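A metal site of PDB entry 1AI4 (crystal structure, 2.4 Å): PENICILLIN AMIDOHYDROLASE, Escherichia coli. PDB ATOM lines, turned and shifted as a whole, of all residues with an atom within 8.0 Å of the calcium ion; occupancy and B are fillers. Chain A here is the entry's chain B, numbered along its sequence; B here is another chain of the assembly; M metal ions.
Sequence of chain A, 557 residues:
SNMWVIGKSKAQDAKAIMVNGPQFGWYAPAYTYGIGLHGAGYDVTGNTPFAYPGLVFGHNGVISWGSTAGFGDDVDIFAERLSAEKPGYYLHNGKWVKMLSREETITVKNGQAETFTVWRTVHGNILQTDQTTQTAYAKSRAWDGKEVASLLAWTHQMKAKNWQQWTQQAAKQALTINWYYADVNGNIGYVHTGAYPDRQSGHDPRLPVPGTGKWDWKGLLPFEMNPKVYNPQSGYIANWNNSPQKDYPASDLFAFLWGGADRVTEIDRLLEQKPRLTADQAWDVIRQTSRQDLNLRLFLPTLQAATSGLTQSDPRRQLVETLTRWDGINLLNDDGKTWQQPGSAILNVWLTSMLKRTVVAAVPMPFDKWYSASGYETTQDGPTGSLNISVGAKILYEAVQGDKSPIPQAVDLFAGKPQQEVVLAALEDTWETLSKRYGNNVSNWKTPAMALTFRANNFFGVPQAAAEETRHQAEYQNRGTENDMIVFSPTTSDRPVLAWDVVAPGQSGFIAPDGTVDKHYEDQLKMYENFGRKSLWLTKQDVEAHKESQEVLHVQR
OD1 of Asp 252 lies within hydrogen-bond range of N of Ser 151 of chain B, 2.7 Å away.
The backbone carbonyl oxygen (O) of Asp 252 lies close to the side-chain amide oxygen (OD1) of Asn 155 of chain B, at 2.9 Å.
N of Ile 77 sits at hydrogen-bond distance from OE1 of Glu 152 of chain B, at 3.0 Å.
The indole nitrogen (NE1) of Trp 217 is in hydrogen-bond range of the side-chain carboxylate (OD2) of Asp 76 (3.1 Å).
The side-chain carboxylate of Asp 76 sits close to a ring nitrogen (NE2) of His 203, at 3.4 Å.
The side-chain carboxylate (OD1) of Asp 252 lies within hydrogen-bond range of the side-chain hydroxyl (OG1) of Thr 150 of chain B (2.9 Å).
The backbone carbonyl oxygen (O) of Asp 73 is in hydrogen-bond range of the guanidinium group (NH2) of Arg 199 (3.3 Å).
The backbone carbonyl oxygen (O) of Asp 76 lies within hydrogen-bond range of the backbone NH (N) of Ser 140 (2.9 Å).
Of the 25 residues printed, 6 come within 4 Å of the calcium ion.
Along chain A the residues within 4 Å of the calcium ion span positions 73 to 252.
The calcium ion is bound by the side-chain carboxylate (OE2) of Glu 152 of chain B.
The calcium ion is bound by OD2 of Asp 252 (2.3 Å).
OD1 of Asp 76 is bound to the calcium ion, 2.3 Å away.
The calcium ion is bound by OD2 of Asp 73, 2.4 Å away.
The calcium ion is bound by OD1 of Asp 73 (2.6 Å).
The calcium ion is bound by O of Pro 205, 2.7 Å away.
O of Val 75 binds the calcium ion, 2.7 Å away.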
ATOM      1  N   GLY A  72      -4.605 -10.833   4.562  1.00  0.00           N
ATOM      2  CA  GLY A  72      -5.260 -12.151   4.823  1.00  0.00           C
ATOM      3  C   GLY A  72      -6.703 -12.023   4.421  1.00  0.00           C
ATOM      4  O   GLY A  72      -7.158 -10.911   4.158  1.00  0.00           O
ATOM      5  N   ASP A  73      -7.474 -13.106   4.388  1.00  0.00           N
ATOM      6  CA  ASP A  73      -8.915 -13.003   4.082  1.00  0.00           C
ATOM      7  C   ASP A  73      -9.689 -12.828   5.409  1.00  0.00           C
ATOM      8  O   ASP A  73      -9.906 -13.740   6.218  1.00  0.00           O
ATOM      9  CB  ASP A  73      -9.457 -14.207   3.323  1.00  0.00           C
ATOM     10  CG  ASP A  73     -10.906 -14.104   2.940  1.00  0.00           C
ATOM     11  OD1 ASP A  73     -11.635 -13.171   3.360  1.00  0.00           O
ATOM     12  OD2 ASP A  73     -11.520 -14.906   2.208  1.00  0.00           O
ATOM     13  N   ASP A  74     -10.091 -11.593   5.704  1.00  0.00           N
ATOM     14  CA  ASP A  74     -10.805 -11.339   6.952  1.00  0.00           C
ATOM     15  C   ASP A  74     -12.175 -10.718   6.726  1.00  0.00           C
ATOM     16  O   ASP A  74     -12.778 -10.092   7.603  1.00  0.00           O
ATOM     17  CB  ASP A  74      -9.952 -10.481   7.892  1.00  0.00           C
ATOM     18  CG  ASP A  74      -9.660  -9.132   7.238  1.00  0.00           C
ATOM     19  OD1 ASP A  74     -10.162  -8.889   6.127  1.00  0.00           O
ATOM     20  OD2 ASP A  74      -8.979  -8.245   7.764  1.00  0.00           O
ATOM     21  N   VAL A  75     -12.602 -10.744   5.465  1.00  0.00           N
ATOM     22  CA  VAL A  75     -13.911 -10.259   5.096  1.00  0.00           C
ATOM     23  C   VAL A  75     -14.685 -11.306   4.295  1.00  0.00           C
ATOM     24  O   VAL A  75     -14.161 -11.599   3.206  1.00  0.00           O
ATOM     25  CB  VAL A  75     -13.709  -8.974   4.262  1.00  0.00           C
ATOM     26  CG1 VAL A  75     -15.041  -8.456   3.753  1.00  0.00           C
ATOM     27  CG2 VAL A  75     -13.016  -7.852   5.025  1.00  0.00           C
ATOM     28  N   ASP A  76     -15.891 -11.753   4.630  1.00  0.00           N
ATOM     29  CA  ASP A  76     -16.747 -12.549   3.769  1.00  0.00           C
ATOM     30  C   ASP A  76     -18.104 -11.897   3.530  1.00  0.00           C
ATOM     31  O   ASP A  76     -18.604 -11.004   4.248  1.00  0.00           O
ATOM     32  CB  ASP A  76     -16.950 -13.985   4.267  1.00  0.00           C
ATOM     33  CG  ASP A  76     -15.722 -14.785   4.556  1.00  0.00           C
ATOM     34  OD1 ASP A  76     -14.632 -14.654   3.933  1.00  0.00           O
ATOM     35  OD2 ASP A  76     -15.791 -15.649   5.479  1.00  0.00           O
ATOM     36  N   ILE A  77     -18.873 -12.372   2.556  1.00  0.00           N
ATOM     37  CA  ILE A  77     -20.122 -11.779   2.094  1.00  0.00           C
ATOM     38  C   ILE A  77     -21.309 -12.701   2.355  1.00  0.00           C
ATOM     39  O   ILE A  77     -21.263 -13.891   2.057  1.00  0.00           O
ATOM     40  CB  ILE A  77     -20.113 -11.419   0.592  1.00  0.00           C
ATOM     41  CG1 ILE A  77     -19.043 -10.423   0.149  1.00  0.00           C
ATOM     42  CG2 ILE A  77     -21.479 -10.901   0.137  1.00  0.00           C
ATOM     43  CD1 ILE A  77     -19.125  -9.028   0.686  1.00  0.00           C
ATOM     44  N   SER A 140     -19.411  -8.736   5.912  1.00  0.00           N
ATOM     45  CA  SER A 140     -19.047  -9.057   7.263  1.00  0.00           C
ATOM     46  C   SER A 140     -17.537  -9.097   7.476  1.00  0.00           C
ATOM     47  O   SER A 140     -16.796  -9.826   6.848  1.00  0.00           O
ATOM     48  CB  SER A 140     -19.832 -10.285   7.697  1.00  0.00           C
ATOM     49  OG  SER A 140     -19.130 -10.965   8.720  1.00  0.00           O
ATOM     50  N   PRO A 197     -11.773 -15.193  10.908  1.00  0.00           N
ATOM     51  CA  PRO A 197     -12.952 -15.954  11.265  1.00  0.00           C
ATOM     52  C   PRO A 197     -12.744 -17.434  11.437  1.00  0.00           C
ATOM     53  O   PRO A 197     -11.824 -18.011  10.878  1.00  0.00           O
ATOM     54  CB  PRO A 197     -13.999 -15.686  10.155  1.00  0.00           C
ATOM     55  CG  PRO A 197     -13.106 -15.257   8.994  1.00  0.00           C
ATOM     56  CD  PRO A 197     -11.862 -14.641   9.558  1.00  0.00           C
ATOM     57  N   ARG A 199     -14.342 -20.579  10.389  1.00  0.00           N
ATOM     58  CA  ARG A 199     -15.375 -20.838   9.411  1.00  0.00           C
ATOM     59  C   ARG A 199     -15.863 -22.268   9.559  1.00  0.00           C
ATOM     60  O   ARG A 199     -15.147 -23.157   9.987  1.00  0.00           O
ATOM     61  CB  ARG A 199     -14.861 -20.526   8.021  1.00  0.00           C
ATOM     62  CG  ARG A 199     -14.716 -19.028   7.733  1.00  0.00           C
ATOM     63  CD  ARG A 199     -14.029 -18.784   6.410  1.00  0.00           C
ATOM     64  NE  ARG A 199     -13.894 -17.415   5.923  1.00  0.00           N
ATOM     65  CZ  ARG A 199     -12.655 -16.881   5.936  1.00  0.00           C
ATOM     66  NH1 ARG A 199     -11.629 -17.552   6.393  1.00  0.00           N
ATOM     67  NH2 ARG A 199     -12.464 -15.659   5.506  1.00  0.00           N
ATOM     68  N   HIS A 203     -16.967 -24.121   3.919  1.00  0.00           N
ATOM     69  CA  HIS A 203     -17.087 -22.723   3.518  1.00  0.00           C
ATOM     70  C   HIS A 203     -15.851 -22.387   2.658  1.00  0.00           C
ATOM     71  O   HIS A 203     -14.706 -22.492   3.129  1.00  0.00           O
ATOM     72  CB  HIS A 203     -17.119 -21.827   4.758  1.00  0.00           C
ATOM     73  CG  HIS A 203     -17.242 -20.357   4.535  1.00  0.00           C
ATOM     74  ND1 HIS A 203     -17.873 -19.532   5.449  1.00  0.00           N
ATOM     75  CD2 HIS A 203     -16.867 -19.526   3.522  1.00  0.00           C
ATOM     76  CE1 HIS A 203     -17.881 -18.282   5.063  1.00  0.00           C
ATOM     77  NE2 HIS A 203     -17.284 -18.268   3.877  1.00  0.00           N
ATOM     78  N   ASP A 204     -16.109 -22.043   1.426  1.00  0.00           N
ATOM     79  CA  ASP A 204     -15.015 -21.671   0.496  1.00  0.00           C
ATOM     80  C   ASP A 204     -14.977 -20.137   0.610  1.00  0.00           C
ATOM     81  O   ASP A 204     -15.959 -19.468   0.267  1.00  0.00           O
ATOM     82  CB  ASP A 204     -15.349 -22.115  -0.912  1.00  0.00           C
ATOM     83  CG  ASP A 204     -14.348 -21.734  -2.000  1.00  0.00           C
ATOM     84  OD1 ASP A 204     -13.616 -20.728  -1.899  1.00  0.00           O
ATOM     85  OD2 ASP A 204     -14.364 -22.489  -3.015  1.00  0.00           O
ATOM     86  N   PRO A 205     -13.920 -19.616   1.180  1.00  0.00           N
ATOM     87  CA  PRO A 205     -13.805 -18.208   1.512  1.00  0.00           C
ATOM     88  C   PRO A 205     -13.696 -17.306   0.305  1.00  0.00           C
ATOM     89  O   PRO A 205     -13.799 -16.103   0.498  1.00  0.00           O
ATOM     90  CB  PRO A 205     -12.617 -18.105   2.496  1.00  0.00           C
ATOM     91  CG  PRO A 205     -11.793 -19.294   2.054  1.00  0.00           C
ATOM     92  CD  PRO A 205     -12.742 -20.382   1.591  1.00  0.00           C
ATOM     93  N   ARG A 206     -13.645 -17.795  -0.945  1.00  0.00           N
ATOM     94  CA  ARG A 206     -13.591 -16.917  -2.104  1.00  0.00           C
ATOM     95  C   ARG A 206     -14.918 -16.500  -2.646  1.00  0.00           C
ATOM     96  O   ARG A 206     -15.024 -15.696  -3.561  1.00  0.00           O
ATOM     97  CB  ARG A 206     -12.824 -17.595  -3.252  1.00  0.00           C
ATOM     98  CG  ARG A 206     -11.348 -17.856  -2.911  1.00  0.00           C
ATOM     99  CD  ARG A 206     -10.794 -19.032  -3.687  1.00  0.00           C
ATOM    100  NE  ARG A 206     -11.610 -20.246  -3.776  1.00  0.00           N
ATOM    101  CZ  ARG A 206     -11.260 -21.285  -4.547  1.00  0.00           C
ATOM    102  NH1 ARG A 206     -10.157 -21.133  -5.282  1.00  0.00           N
ATOM    103  NH2 ARG A 206     -11.994 -22.392  -4.562  1.00  0.00           N
ATOM    104  N   LEU A 207     -16.003 -17.123  -2.164  1.00  0.00           N
ATOM    105  CA  LEU A 207     -17.338 -16.862  -2.719  1.00  0.00           C
ATOM    106  C   LEU A 207     -18.349 -16.630  -1.611  1.00  0.00           C
ATOM    107  O   LEU A 207     -18.225 -17.183  -0.512  1.00  0.00           O
ATOM    108  CB  LEU A 207     -17.679 -18.154  -3.494  1.00  0.00           C
ATOM    109  CG  LEU A 207     -16.798 -18.502  -4.722  1.00  0.00           C
ATOM    110  CD1 LEU A 207     -16.797 -19.981  -4.987  1.00  0.00           C
ATOM    111  CD2 LEU A 207     -17.273 -17.690  -5.904  1.00  0.00           C
ATOM    112  N   PRO A 208     -19.477 -16.046  -1.915  1.00  0.00           N
ATOM    113  CA  PRO A 208     -20.513 -15.724  -0.926  1.00  0.00           C
ATOM    114  C   PRO A 208     -21.129 -16.901  -0.195  1.00  0.00           C
ATOM    115  O   PRO A 208     -21.157 -18.017  -0.715  1.00  0.00           O
ATOM    116  CB  PRO A 208     -21.623 -14.920  -1.687  1.00  0.00           C
ATOM    117  CG  PRO A 208     -20.861 -14.407  -2.865  1.00  0.00           C
ATOM    118  CD  PRO A 208     -19.699 -15.361  -3.187  1.00  0.00           C
ATOM    119  N   TRP A 217     -20.179 -17.706  10.863  1.00  0.00           N
ATOM    120  CA  TRP A 217     -18.905 -18.029  11.500  1.00  0.00           C
ATOM    121  C   TRP A 217     -19.183 -18.583  12.901  1.00  0.00           C
ATOM    122  O   TRP A 217     -20.218 -18.329  13.531  1.00  0.00           O
ATOM    123  CB  TRP A 217     -17.975 -16.844  11.627  1.00  0.00           C
ATOM    124  CG  TRP A 217     -17.662 -16.081  10.375  1.00  0.00           C
ATOM    125  CD1 TRP A 217     -17.604 -16.590   9.094  1.00  0.00           C
ATOM    126  CD2 TRP A 217     -17.257 -14.713  10.296  1.00  0.00           C
ATOM    127  NE1 TRP A 217     -17.278 -15.577   8.235  1.00  0.00           N
ATOM    128  CE2 TRP A 217     -17.031 -14.437   8.924  1.00  0.00           C
ATOM    129  CE3 TRP A 217     -17.082 -13.684  11.234  1.00  0.00           C
ATOM    130  CZ2 TRP A 217     -16.608 -13.192   8.466  1.00  0.00           C
ATOM    131  CZ3 TRP A 217     -16.688 -12.435  10.768  1.00  0.00           C
ATOM    132  CH2 TRP A 217     -16.454 -12.187   9.399  1.00  0.00           C
ATOM    133  N   ALA A 250      -4.700 -16.201   1.157  1.00  0.00           N
ATOM    134  CA  ALA A 250      -4.679 -14.773   0.946  1.00  0.00           C
ATOM    135  C   ALA A 250      -6.088 -14.227   0.830  1.00  0.00           C
ATOM    136  O   ALA A 250      -7.064 -14.970   0.658  1.00  0.00           O
ATOM    137  CB  ALA A 250      -3.992 -14.531  -0.418  1.00  0.00           C
ATOM    138  N   SER A 251      -6.155 -12.903   0.770  1.00  0.00           N
ATOM    139  CA  SER A 251      -7.367 -12.154   0.542  1.00  0.00           C
ATOM    140  C   SER A 251      -8.107 -12.858  -0.586  1.00  0.00           C
ATOM    141  O   SER A 251      -7.419 -13.327  -1.503  1.00  0.00           O
ATOM    142  CB  SER A 251      -6.892 -10.796  -0.005  1.00  0.00           C
ATOM    143  OG  SER A 251      -8.006 -10.022  -0.346  1.00  0.00           O
ATOM    144  N   ASP A 252      -9.421 -12.756  -0.688  1.00  0.00           N
ATOM    145  CA  ASP A 252     -10.210 -13.281  -1.768  1.00  0.00           C
ATOM    146  C   ASP A 252     -10.228 -12.387  -3.015  1.00  0.00           C
ATOM    147  O   ASP A 252     -10.852 -12.791  -4.013  1.00  0.00           O
ATOM    148  CB  ASP A 252     -11.654 -13.579  -1.325  1.00  0.00           C
ATOM    149  CG  ASP A 252     -12.472 -12.380  -0.862  1.00  0.00           C
ATOM    150  OD1 ASP A 252     -12.592 -11.370  -1.615  1.00  0.00           O
ATOM    151  OD2 ASP A 252     -13.053 -12.463   0.253  1.00  0.00           O
ATOM    152  N   LEU A 253      -9.522 -11.269  -3.015  1.00  0.00           N
ATOM    153  CA  LEU A 253      -9.495 -10.418  -4.209  1.00  0.00           C
ATOM    154  C   LEU A 253      -9.079 -11.204  -5.487  1.00  0.00           C
ATOM    155  O   LEU A 253      -8.020 -11.843  -5.450  1.00  0.00           O
ATOM    156  CB  LEU A 253      -8.435  -9.310  -4.073  1.00  0.00           C
ATOM    157  CG  LEU A 253      -8.877  -8.094  -3.295  1.00  0.00           C
ATOM    158  CD1 LEU A 253      -7.683  -7.142  -3.164  1.00  0.00           C
ATOM    159  CD2 LEU A 253     -10.066  -7.427  -3.984  1.00  0.00           C
ATOM    160  N   SER B 149     -10.722  -5.591   2.137  1.00  0.00           N
ATOM    161  CA  SER B 149     -10.697  -5.968   0.720  1.00  0.00           C
ATOM    162  C   SER B 149     -11.484  -7.213   0.406  1.00  0.00           C
ATOM    163  O   SER B 149     -11.116  -8.241   1.005  1.00  0.00           O
ATOM    164  CB  SER B 149      -9.242  -6.287   0.307  1.00  0.00           C
ATOM    165  OG  SER B 149      -8.409  -5.162   0.413  1.00  0.00           O
ATOM    166  N   THR B 150     -12.450  -7.181  -0.486  1.00  0.00           N
ATOM    167  CA  THR B 150     -13.130  -8.436  -0.838  1.00  0.00           C
ATOM    168  C   THR B 150     -13.594  -8.284  -2.289  1.00  0.00           C
ATOM    169  O   THR B 150     -13.922  -7.163  -2.667  1.00  0.00           O
ATOM    170  CB  THR B 150     -14.331  -8.781   0.066  1.00  0.00           C
ATOM    171  OG1 THR B 150     -14.860 -10.104  -0.231  1.00  0.00           O
ATOM    172  CG2 THR B 150     -15.543  -7.869  -0.168  1.00  0.00           C
ATOM    173  N   SER B 151     -13.829  -9.357  -3.014  1.00  0.00           N
ATOM    174  CA  SER B 151     -14.389  -9.258  -4.362  1.00  0.00           C
ATOM    175  C   SER B 151     -15.253 -10.516  -4.566  1.00  0.00           C
ATOM    176  O   SER B 151     -15.505 -10.846  -5.711  1.00  0.00           O
ATOM    177  CB  SER B 151     -13.363  -9.178  -5.509  1.00  0.00           C
ATOM    178  OG  SER B 151     -12.637 -10.378  -5.722  1.00  0.00           O
ATOM    179  N   GLU B 152     -15.853 -11.005  -3.464  1.00  0.00           N
ATOM    180  CA  GLU B 152     -16.582 -12.249  -3.492  1.00  0.00           C
ATOM    181  C   GLU B 152     -17.753 -12.241  -4.463  1.00  0.00           C
ATOM    182  O   GLU B 152     -18.041 -13.256  -5.137  1.00  0.00           O
ATOM    183  CB  GLU B 152     -17.010 -12.781  -2.133  1.00  0.00           C
ATOM    184  CG  GLU B 152     -15.896 -13.323  -1.244  1.00  0.00           C
ATOM    185  CD  GLU B 152     -16.464 -13.701   0.133  1.00  0.00           C
ATOM    186  OE1 GLU B 152     -17.725 -13.847   0.174  1.00  0.00           O
ATOM    187  OE2 GLU B 152     -15.697 -13.888   1.124  1.00  0.00           O
ATOM    188  N   ASN B 155     -16.138 -12.553  -7.884  1.00  0.00           N
ATOM    189  CA  ASN B 155     -15.731 -13.912  -8.076  1.00  0.00           C
ATOM    190  C   ASN B 155     -16.862 -14.851  -8.472  1.00  0.00           C
ATOM    191  O   ASN B 155     -16.668 -15.715  -9.337  1.00  0.00           O
ATOM    192  CB  ASN B 155     -14.971 -14.414  -6.877  1.00  0.00           C
ATOM    193  CG  ASN B 155     -13.768 -13.505  -6.640  1.00  0.00           C
ATOM    194  OD1 ASN B 155     -13.121 -13.690  -5.603  1.00  0.00           O
ATOM    195  ND2 ASN B 155     -13.427 -12.525  -7.436  1.00  0.00           N
HETATM  196 CA    CA M   1     -13.649 -13.883   1.944  1.00  0.00          CA
